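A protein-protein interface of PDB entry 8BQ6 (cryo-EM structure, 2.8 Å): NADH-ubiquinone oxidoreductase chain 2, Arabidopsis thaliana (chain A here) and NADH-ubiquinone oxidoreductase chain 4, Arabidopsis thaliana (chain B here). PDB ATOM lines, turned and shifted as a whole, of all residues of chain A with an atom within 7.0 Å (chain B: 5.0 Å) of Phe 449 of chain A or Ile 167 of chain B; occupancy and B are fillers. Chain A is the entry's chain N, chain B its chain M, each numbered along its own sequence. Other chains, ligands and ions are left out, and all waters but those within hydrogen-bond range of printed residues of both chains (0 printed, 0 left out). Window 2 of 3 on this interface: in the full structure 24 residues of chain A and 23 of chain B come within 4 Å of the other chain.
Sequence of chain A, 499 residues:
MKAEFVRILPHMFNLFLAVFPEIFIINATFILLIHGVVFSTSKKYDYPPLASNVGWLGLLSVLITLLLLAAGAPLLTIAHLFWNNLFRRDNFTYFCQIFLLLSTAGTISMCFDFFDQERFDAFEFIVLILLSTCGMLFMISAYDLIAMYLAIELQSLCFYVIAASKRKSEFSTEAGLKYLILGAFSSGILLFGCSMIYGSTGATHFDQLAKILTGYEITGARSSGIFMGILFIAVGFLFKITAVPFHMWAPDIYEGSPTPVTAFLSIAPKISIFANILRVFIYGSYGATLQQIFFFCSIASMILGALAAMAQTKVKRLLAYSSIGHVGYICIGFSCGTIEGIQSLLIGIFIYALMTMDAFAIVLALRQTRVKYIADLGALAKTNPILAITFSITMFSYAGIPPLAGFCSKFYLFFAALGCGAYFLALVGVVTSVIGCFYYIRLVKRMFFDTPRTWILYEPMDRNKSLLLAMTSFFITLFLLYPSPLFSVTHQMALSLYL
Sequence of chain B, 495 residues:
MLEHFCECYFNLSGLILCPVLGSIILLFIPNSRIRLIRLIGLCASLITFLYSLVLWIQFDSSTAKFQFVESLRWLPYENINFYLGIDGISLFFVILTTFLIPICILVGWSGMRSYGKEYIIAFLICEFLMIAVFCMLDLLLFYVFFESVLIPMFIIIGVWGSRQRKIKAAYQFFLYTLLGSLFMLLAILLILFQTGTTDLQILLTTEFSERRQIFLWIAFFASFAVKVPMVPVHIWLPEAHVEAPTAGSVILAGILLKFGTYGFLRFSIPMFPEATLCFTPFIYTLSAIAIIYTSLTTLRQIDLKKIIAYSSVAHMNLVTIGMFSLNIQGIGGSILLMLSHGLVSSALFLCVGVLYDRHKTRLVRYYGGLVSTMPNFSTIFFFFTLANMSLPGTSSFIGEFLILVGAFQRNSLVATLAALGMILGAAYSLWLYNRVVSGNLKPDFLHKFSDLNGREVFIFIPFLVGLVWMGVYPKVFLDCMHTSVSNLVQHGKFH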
ATOM      1  N   ALA A 379       0.541  10.463  11.641  1.00  0.00           N
ATOM      2  CA  ALA A 379      -0.361  10.918  12.698  1.00  0.00           C
ATOM      3  C   ALA A 379      -1.386   9.865  13.098  1.00  0.00           C
ATOM      4  O   ALA A 379      -2.498  10.209  13.506  1.00  0.00           O
ATOM      5  CB  ALA A 379      -1.075  12.217  12.306  1.00  0.00           C
ATOM      6  N   ALA A 381      -0.991   7.965  15.654  1.00  0.00           N
ATOM      7  CA  ALA A 381      -1.002   7.957  17.109  1.00  0.00           C
ATOM      8  C   ALA A 381      -1.937   9.015  17.679  1.00  0.00           C
ATOM      9  O   ALA A 381      -2.292   8.942  18.860  1.00  0.00           O
ATOM     10  CB  ALA A 381       0.415   8.148  17.640  1.00  0.00           C
ATOM     11  N   ILE A 441      11.549   0.499  12.862  1.00  0.00           N
ATOM     12  CA  ILE A 441      11.294   1.694  13.666  1.00  0.00           C
ATOM     13  C   ILE A 441      10.994   2.914  12.812  1.00  0.00           C
ATOM     14  O   ILE A 441      10.493   3.915  13.338  1.00  0.00           O
ATOM     15  CB  ILE A 441      12.459   2.009  14.627  1.00  0.00           C
ATOM     16  CG1 ILE A 441      13.711   2.437  13.862  1.00  0.00           C
ATOM     17  CG2 ILE A 441      12.746   0.825  15.538  1.00  0.00           C
ATOM     18  CD1 ILE A 441      14.806   2.976  14.752  1.00  0.00           C
ATOM     19  N   LEU A 443       8.592   2.916  10.719  1.00  0.00           N
ATOM     20  CA  LEU A 443       7.107   2.975  10.787  1.00  0.00           C
ATOM     21  C   LEU A 443       6.669   3.599  12.116  1.00  0.00           C
ATOM     22  O   LEU A 443       5.713   4.370  12.096  1.00  0.00           O
ATOM     23  CB  LEU A 443       6.510   1.576  10.609  1.00  0.00           C
ATOM     24  CG  LEU A 443       6.148   1.212   9.172  1.00  0.00           C
ATOM     25  CD1 LEU A 443       7.400   0.971   8.350  1.00  0.00           C
ATOM     26  CD2 LEU A 443       5.241  -0.004   9.130  1.00  0.00           C
ATOM     27  N   VAL A 444       7.330   3.258  13.224  1.00  0.00           N
ATOM     28  CA  VAL A 444       6.980   3.854  14.509  1.00  0.00           C
ATOM     29  C   VAL A 444       7.225   5.357  14.476  1.00  0.00           C
ATOM     30  O   VAL A 444       6.432   6.146  15.009  1.00  0.00           O
ATOM     31  CB  VAL A 444       7.762   3.161  15.639  1.00  0.00           C
ATOM     32  CG1 VAL A 444       7.464   3.807  16.972  1.00  0.00           C
ATOM     33  CG2 VAL A 444       7.403   1.686  15.675  1.00  0.00           C
ATOM     34  N   LYS A 445       8.312   5.776  13.827  1.00  0.00           N
ATOM     35  CA  LYS A 445       8.560   7.199  13.632  1.00  0.00           C
ATOM     36  C   LYS A 445       7.448   7.847  12.816  1.00  0.00           C
ATOM     37  O   LYS A 445       6.988   8.946  13.143  1.00  0.00           O
ATOM     38  CB  LYS A 445       9.912   7.401  12.952  1.00  0.00           C
ATOM     39  CG  LYS A 445      10.115   8.783  12.368  1.00  0.00           C
ATOM     40  CD  LYS A 445       9.883   8.807  10.870  1.00  0.00           C
ATOM     41  CE  LYS A 445      10.250  10.155  10.299  1.00  0.00           C
ATOM     42  NZ  LYS A 445       9.734  10.322   8.915  1.00  0.00           N
ATOM     43  N   ARG A 446       7.013   7.186  11.740  1.00  0.00           N
ATOM     44  CA  ARG A 446       5.950   7.751  10.918  1.00  0.00           C
ATOM     45  C   ARG A 446       4.660   7.914  11.713  1.00  0.00           C
ATOM     46  O   ARG A 446       3.966   8.929  11.585  1.00  0.00           O
ATOM     47  CB  ARG A 446       5.709   6.879   9.690  1.00  0.00           C
ATOM     48  CG  ARG A 446       4.620   7.404   8.783  1.00  0.00           C
ATOM     49  CD  ARG A 446       5.000   8.757   8.225  1.00  0.00           C
ATOM     50  NE  ARG A 446       6.070   8.657   7.240  1.00  0.00           N
ATOM     51  CZ  ARG A 446       6.388   9.616   6.382  1.00  0.00           C
ATOM     52  NH1 ARG A 446       5.737  10.767   6.361  1.00  0.00           N
ATOM     53  NH2 ARG A 446       7.376   9.411   5.517  1.00  0.00           N
ATOM     54  N   MET A 447       4.322   6.950  12.559  1.00  0.00           N
ATOM     55  CA  MET A 447       3.029   7.026  13.279  1.00  0.00           C
ATOM     56  C   MET A 447       3.116   7.956  14.488  1.00  0.00           C
ATOM     57  O   MET A 447       2.071   8.482  14.872  1.00  0.00           O
ATOM     58  CB  MET A 447       2.608   5.647  13.792  1.00  0.00           C
ATOM     59  CG  MET A 447       2.260   4.660  12.705  1.00  0.00           C
ATOM     60  SD  MET A 447       1.705   3.100  13.422  1.00  0.00           S
ATOM     61  CE  MET A 447       3.272   2.366  13.886  1.00  0.00           C
ATOM     62  N   PHE A 448       4.309   8.180  15.043  1.00  0.00           N
ATOM     63  CA  PHE A 448       4.385   8.918  16.295  1.00  0.00           C
ATOM     64  C   PHE A 448       5.085  10.260  16.191  1.00  0.00           C
ATOM     65  O   PHE A 448       4.628  11.223  16.807  1.00  0.00           O
ATOM     66  CB  PHE A 448       5.086   8.059  17.356  1.00  0.00           C
ATOM     67  CG  PHE A 448       4.172   7.093  18.043  1.00  0.00           C
ATOM     68  CD1 PHE A 448       4.033   5.801  17.568  1.00  0.00           C
ATOM     69  CD2 PHE A 448       3.482   7.459  19.181  1.00  0.00           C
ATOM     70  CE1 PHE A 448       3.196   4.907  18.191  1.00  0.00           C
ATOM     71  CE2 PHE A 448       2.652   6.562  19.814  1.00  0.00           C
ATOM     72  CZ  PHE A 448       2.509   5.283  19.313  1.00  0.00           C
ATOM     73  N   PHE A 449       6.160  10.365  15.413  1.00  0.00           N
ATOM     74  CA  PHE A 449       6.998  11.554  15.455  1.00  0.00           C
ATOM     75  C   PHE A 449       6.673  12.564  14.364  1.00  0.00           C
ATOM     76  O   PHE A 449       7.033  13.737  14.496  1.00  0.00           O
ATOM     77  CB  PHE A 449       8.485  11.177  15.354  1.00  0.00           C
ATOM     78  CG  PHE A 449       8.917  10.061  16.278  1.00  0.00           C
ATOM     79  CD1 PHE A 449       8.161   9.698  17.381  1.00  0.00           C
ATOM     80  CD2 PHE A 449      10.105   9.391  16.050  1.00  0.00           C
ATOM     81  CE1 PHE A 449       8.566   8.678  18.213  1.00  0.00           C
ATOM     82  CE2 PHE A 449      10.516   8.376  16.885  1.00  0.00           C
ATOM     83  CZ  PHE A 449       9.746   8.019  17.968  1.00  0.00           C
ATOM     84  N   ASP A 450       5.997  12.151  13.300  1.00  0.00           N
ATOM     85  CA  ASP A 450       5.797  13.037  12.165  1.00  0.00           C
ATOM     86  C   ASP A 450       4.584  13.929  12.382  1.00  0.00           C
ATOM     87  O   ASP A 450       3.630  13.564  13.073  1.00  0.00           O
ATOM     88  CB  ASP A 450       5.624  12.225  10.885  1.00  0.00           C
ATOM     89  CG  ASP A 450       6.940  11.925  10.210  1.00  0.00           C
ATOM     90  OD1 ASP A 450       7.785  12.838  10.110  1.00  0.00           O
ATOM     91  OD2 ASP A 450       7.132  10.770   9.783  1.00  0.00           O
ATOM     92  N   THR A 451       4.626  15.114  11.776  1.00  0.00           N
ATOM     93  CA  THR A 451       3.515  16.065  11.806  1.00  0.00           C
ATOM     94  C   THR A 451       3.157  16.432  10.372  1.00  0.00           C
ATOM     95  O   THR A 451       3.556  17.489   9.866  1.00  0.00           O
ATOM     96  CB  THR A 451       3.855  17.310  12.632  1.00  0.00           C
ATOM     97  OG1 THR A 451       5.128  17.833  12.234  1.00  0.00           O
ATOM     98  CG2 THR A 451       3.875  16.986  14.116  1.00  0.00           C
ATOM     99  N   PRO A 452       2.395  15.579   9.690  1.00  0.00           N
ATOM    100  CA  PRO A 452       2.040  15.858   8.296  1.00  0.00           C
ATOM    101  C   PRO A 452       1.013  16.973   8.183  1.00  0.00           C
ATOM    102  O   PRO A 452       0.243  17.255   9.104  1.00  0.00           O
ATOM    103  CB  PRO A 452       1.461  14.531   7.792  1.00  0.00           C
ATOM    104  CG  PRO A 452       1.248  13.679   8.997  1.00  0.00           C
ATOM    105  CD  PRO A 452       1.679  14.412  10.224  1.00  0.00           C
ATOM    106  N   PHE B 154      13.131   5.794  22.951  1.00  0.00           N
ATOM    107  CA  PHE B 154      12.853   6.173  21.570  1.00  0.00           C
ATOM    108  C   PHE B 154      11.552   6.955  21.470  1.00  0.00           C
ATOM    109  O   PHE B 154      11.496   8.024  20.845  1.00  0.00           O
ATOM    110  CB  PHE B 154      12.794   4.888  20.737  1.00  0.00           C
ATOM    111  CG  PHE B 154      12.610   5.094  19.264  1.00  0.00           C
ATOM    112  CD1 PHE B 154      13.596   5.683  18.500  1.00  0.00           C
ATOM    113  CD2 PHE B 154      11.467   4.632  18.634  1.00  0.00           C
ATOM    114  CE1 PHE B 154      13.432   5.838  17.142  1.00  0.00           C
ATOM    115  CE2 PHE B 154      11.297   4.788  17.277  1.00  0.00           C
ATOM    116  CZ  PHE B 154      12.280   5.391  16.530  1.00  0.00           C
ATOM    117  N   ILE B 155      10.492   6.432  22.095  1.00  0.00           N
ATOM    118  CA  ILE B 155       9.206   7.125  22.074  1.00  0.00           C
ATOM    119  C   ILE B 155       9.332   8.508  22.704  1.00  0.00           C
ATOM    120  O   ILE B 155       8.889   9.511  22.131  1.00  0.00           O
ATOM    121  CB  ILE B 155       8.133   6.277  22.783  1.00  0.00           C
ATOM    122  CG1 ILE B 155       7.895   4.959  22.039  1.00  0.00           C
ATOM    123  CG2 ILE B 155       6.838   7.060  22.924  1.00  0.00           C
ATOM    124  CD1 ILE B 155       7.460   5.126  20.608  1.00  0.00           C
ATOM    125  N   GLY B 158      11.348  10.955  20.425  1.00  0.00           N
ATOM    126  CA  GLY B 158      10.718  11.305  19.161  1.00  0.00           C
ATOM    127  C   GLY B 158       9.427  12.091  19.303  1.00  0.00           C
ATOM    128  O   GLY B 158       9.171  13.019  18.532  1.00  0.00           O
ATOM    129  N   VAL B 159       8.576  11.713  20.257  1.00  0.00           N
ATOM    130  CA  VAL B 159       7.261  12.338  20.347  1.00  0.00           C
ATOM    131  C   VAL B 159       7.357  13.735  20.949  1.00  0.00           C
ATOM    132  O   VAL B 159       6.811  14.699  20.404  1.00  0.00           O
ATOM    133  CB  VAL B 159       6.297  11.433  21.137  1.00  0.00           C
ATOM    134  CG1 VAL B 159       4.971  12.128  21.359  1.00  0.00           C
ATOM    135  CG2 VAL B 159       6.073  10.133  20.385  1.00  0.00           C
ATOM    136  N   ARG B 163      12.090  19.894  18.265  1.00  0.00           N
ATOM    137  CA  ARG B 163      12.223  20.186  16.844  1.00  0.00           C
ATOM    138  C   ARG B 163      12.588  18.918  16.088  1.00  0.00           C
ATOM    139  O   ARG B 163      12.960  17.901  16.676  1.00  0.00           O
ATOM    140  CB  ARG B 163      13.251  21.292  16.602  1.00  0.00           C
ATOM    141  CG  ARG B 163      14.627  20.975  17.115  1.00  0.00           C
ATOM    142  CD  ARG B 163      15.570  22.099  16.729  1.00  0.00           C
ATOM    143  NE  ARG B 163      16.949  21.869  17.139  1.00  0.00           N
ATOM    144  CZ  ARG B 163      17.939  22.734  16.964  1.00  0.00           C
ATOM    145  NH1 ARG B 163      17.736  23.915  16.405  1.00  0.00           N
ATOM    146  NH2 ARG B 163      19.170  22.397  17.344  1.00  0.00           N
ATOM    147  N   GLN B 164      12.494  18.994  14.759  1.00  0.00           N
ATOM    148  CA  GLN B 164      12.499  17.789  13.938  1.00  0.00           C
ATOM    149  C   GLN B 164      13.866  17.123  13.832  1.00  0.00           C
ATOM    150  O   GLN B 164      13.962  16.065  13.203  1.00  0.00           O
ATOM    151  CB  GLN B 164      11.976  18.096  12.537  1.00  0.00           C
ATOM    152  CG  GLN B 164      12.646  19.270  11.868  1.00  0.00           C
ATOM    153  CD  GLN B 164      13.567  18.832  10.752  1.00  0.00           C
ATOM    154  OE1 GLN B 164      13.309  17.836  10.077  1.00  0.00           O
ATOM    155  NE2 GLN B 164      14.654  19.568  10.558  1.00  0.00           N
ATOM    156  N   ARG B 165      14.892  17.705  14.453  1.00  0.00           N
ATOM    157  CA  ARG B 165      16.198  17.006  14.512  1.00  0.00           C
ATOM    158  C   ARG B 165      16.038  15.803  15.448  1.00  0.00           C
ATOM    159  O   ARG B 165      16.906  14.925  15.405  1.00  0.00           O
ATOM    160  CB  ARG B 165      17.302  17.965  14.963  1.00  0.00           C
ATOM    161  CG  ARG B 165      17.635  19.057  13.958  1.00  0.00           C
ATOM    162  CD  ARG B 165      18.992  19.677  14.223  1.00  0.00           C
ATOM    163  NE  ARG B 165      20.018  19.187  13.311  1.00  0.00           N
ATOM    164  CZ  ARG B 165      20.977  18.328  13.637  1.00  0.00           C
ATOM    165  NH1 ARG B 165      21.859  17.947  12.728  1.00  0.00           N
ATOM    166  NH2 ARG B 165      21.056  17.850  14.867  1.00  0.00           N
ATOM    167  N   LYS B 166      14.973  15.764  16.259  1.00  0.00           N
ATOM    168  CA  LYS B 166      14.694  14.620  17.114  1.00  0.00           C
ATOM    169  C   LYS B 166      14.549  13.330  16.311  1.00  0.00           C
ATOM    170  O   LYS B 166      14.839  12.252  16.835  1.00  0.00           O
ATOM    171  CB  LYS B 166      13.437  14.890  17.942  1.00  0.00           C
ATOM    172  CG  LYS B 166      12.155  14.883  17.132  1.00  0.00           C
ATOM    173  CD  LYS B 166      11.048  15.663  17.806  1.00  0.00           C
ATOM    174  CE  LYS B 166       9.867  15.810  16.868  1.00  0.00           C
ATOM    175  NZ  LYS B 166       8.571  15.767  17.581  1.00  0.00           N
ATOM    176  N   ILE B 167      14.119  13.409  15.046  1.00  0.00           N
ATOM    177  CA  ILE B 167      14.019  12.206  14.213  1.00  0.00           C
ATOM    178  C   ILE B 167      15.378  11.521  14.115  1.00  0.00           C
ATOM    179  O   ILE B 167      15.555  10.357  14.511  1.00  0.00           O
ATOM    180  CB  ILE B 167      13.487  12.558  12.811  1.00  0.00           C
ATOM    181  CG1 ILE B 167      12.159  13.313  12.877  1.00  0.00           C
ATOM    182  CG2 ILE B 167      13.327  11.303  11.976  1.00  0.00           C
ATOM    183  CD1 ILE B 167      11.009  12.465  13.287  1.00  0.00           C
ATOM    184  N   LYS B 168      16.353  12.251  13.568  1.00  0.00           N
ATOM    185  CA  LYS B 168      17.714  11.753  13.436  1.00  0.00           C
ATOM    186  C   LYS B 168      18.277  11.331  14.787  1.00  0.00           C
ATOM    187  O   LYS B 168      18.935  10.286  14.896  1.00  0.00           O
ATOM    188  CB  LYS B 168      18.570  12.846  12.791  1.00  0.00           C
ATOM    189  CG  LYS B 168      20.069  12.706  12.929  1.00  0.00           C
ATOM    190  CD  LYS B 168      20.692  12.049  11.712  1.00  0.00           C
ATOM    191  CE  LYS B 168      21.943  12.807  11.283  1.00  0.00           C
ATOM    192  NZ  LYS B 168      22.787  13.205  12.447  1.00  0.00           N
ATOM    193  N   ALA B 169      18.009  12.120  15.832  1.00  0.00           N
ATOM    194  CA  ALA B 169      18.552  11.813  17.153  1.00  0.00           C
ATOM    195  C   ALA B 169      18.044  10.470  17.670  1.00  0.00           C
ATOM    196  O   ALA B 169      18.820   9.649  18.181  1.00  0.00           O
ATOM    197  CB  ALA B 169      18.198  12.933  18.131  1.00  0.00           C
ATOM    198  N   ALA B 170      16.735  10.236  17.557  1.00  0.00           N
ATOM    199  CA  ALA B 170      16.147   8.990  18.033  1.00  0.00           C
ATOM    200  C   ALA B 170      16.658   7.801  17.233  1.00  0.00           C
ATOM    201  O   ALA B 170      16.957   6.742  17.806  1.00  0.00           O
ATOM    202  CB  ALA B 170      14.623   9.078  17.969  1.00  0.00           C
ATOM    203  N   TYR B 171      16.778   7.962  15.911  1.00  0.00           N
ATOM    204  CA  TYR B 171      17.356   6.899  15.092  1.00  0.00           C
ATOM    205  C   TYR B 171      18.752   6.531  15.573  1.00  0.00           C
ATOM    206  O   TYR B 171      19.066   5.350  15.774  1.00  0.00           O
ATOM    207  CB  TYR B 171      17.426   7.333  13.631  1.00  0.00           C
ATOM    208  CG  TYR B 171      16.139   7.197  12.869  1.00  0.00           C
ATOM    209  CD1 TYR B 171      15.240   6.183  13.151  1.00  0.00           C
ATOM    210  CD2 TYR B 171      15.826   8.092  11.862  1.00  0.00           C
ATOM    211  CE1 TYR B 171      14.065   6.068  12.449  1.00  0.00           C
ATOM    212  CE2 TYR B 171      14.661   7.984  11.159  1.00  0.00           C
ATOM    213  CZ  TYR B 171      13.783   6.975  11.454  1.00  0.00           C
ATOM    214  OH  TYR B 171      12.619   6.879  10.740  1.00  0.00           O
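The backbone carbonyl oxygen (O) of Val 159 of chain B is in hydrogen-bond range of the side-chain amino group (NZ) of Lys 166 of chain B (3.5 Å).
OD2 of Asp 450 of chain A lies within salt-bridge range of NZ of Lys 445 of chain A (2.8 Å).
O of Gly 158 of chain B is in hydrogen-bond range of NZ of Lys 166 of chain B, 3.0 Å away.
Among the printed residues, merely in contact across the chains: Phe 449 of chain A with Gly 158 of chain B (3.3 Å), Lys 445 of chain A with Tyr 171 of chain B (3.3 Å), Phe 449 of chain A with Phe 154 of chain B (3.4 Å), Phe 449 of chain A with Ile 167 of chain B (3.5 Å), Phe 449 of chain A with Val 159 of chain B (3.5 Å), Ile 441 of chain A with Tyr 171 of chain B (3.6 Å), Lys 445 of chain A with Ile 167 of chain B (3.7 Å), Phe 448 of chain A with Val 159 of chain B (3.8 Å), Val 444 of chain A with Ile 155 of chain B (3.9 Å), Ile 441 of chain A with Phe 154 of chain B (3.9 Å) and Val 444 of chain A with Phe 154 of chain B (3.97 Å).
Of the printed residues of chain B, Ile 441 of chain A touches Phe 154 (3.9 Å) and Tyr 171 (3.6 Å).
Of the printed residues of chain B, Phe 449 of chain A touches Phe 154 (3.4 Å), Gly 158 (3.3 Å), Val 159 (3.5 Å) and Ile 167 (3.5 Å).
Pro 452 of chain A touches none of the printed residues of chain B.
Printed residues of chain A within 4 Å of Phe 154 of chain B: Ile 441, Val 444 and Phe 449.
Printed residues of chain A within 4 Å of Gly 158 of chain B: Phe 449 (3.3 Å).
Arg 163 of chain B touches none of the printed residues of chain A.
Ile 167 of chain B touches two residues of chain A.
Of the printed residues of chain A, Tyr 171 of chain B touches Ile 441 and Lys 445.
Printed residues of chain A that touch a printed residue of chain B: Ile 441, Val 444, Lys 445, Phe 448 and Phe 449.
Along chain A the printed residues that touch a printed residue of chain B span positions 441 to 449.
Of the 13 printed residues of chain B, 6 touch a printed residue of chain A.
Among the printed residues, 11 pairs touch across the chains.
Among the printed residues, no Asp or Glu carboxylate lies within 4 Å of a Lys or Arg side-chain nitrogen of the other chain.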
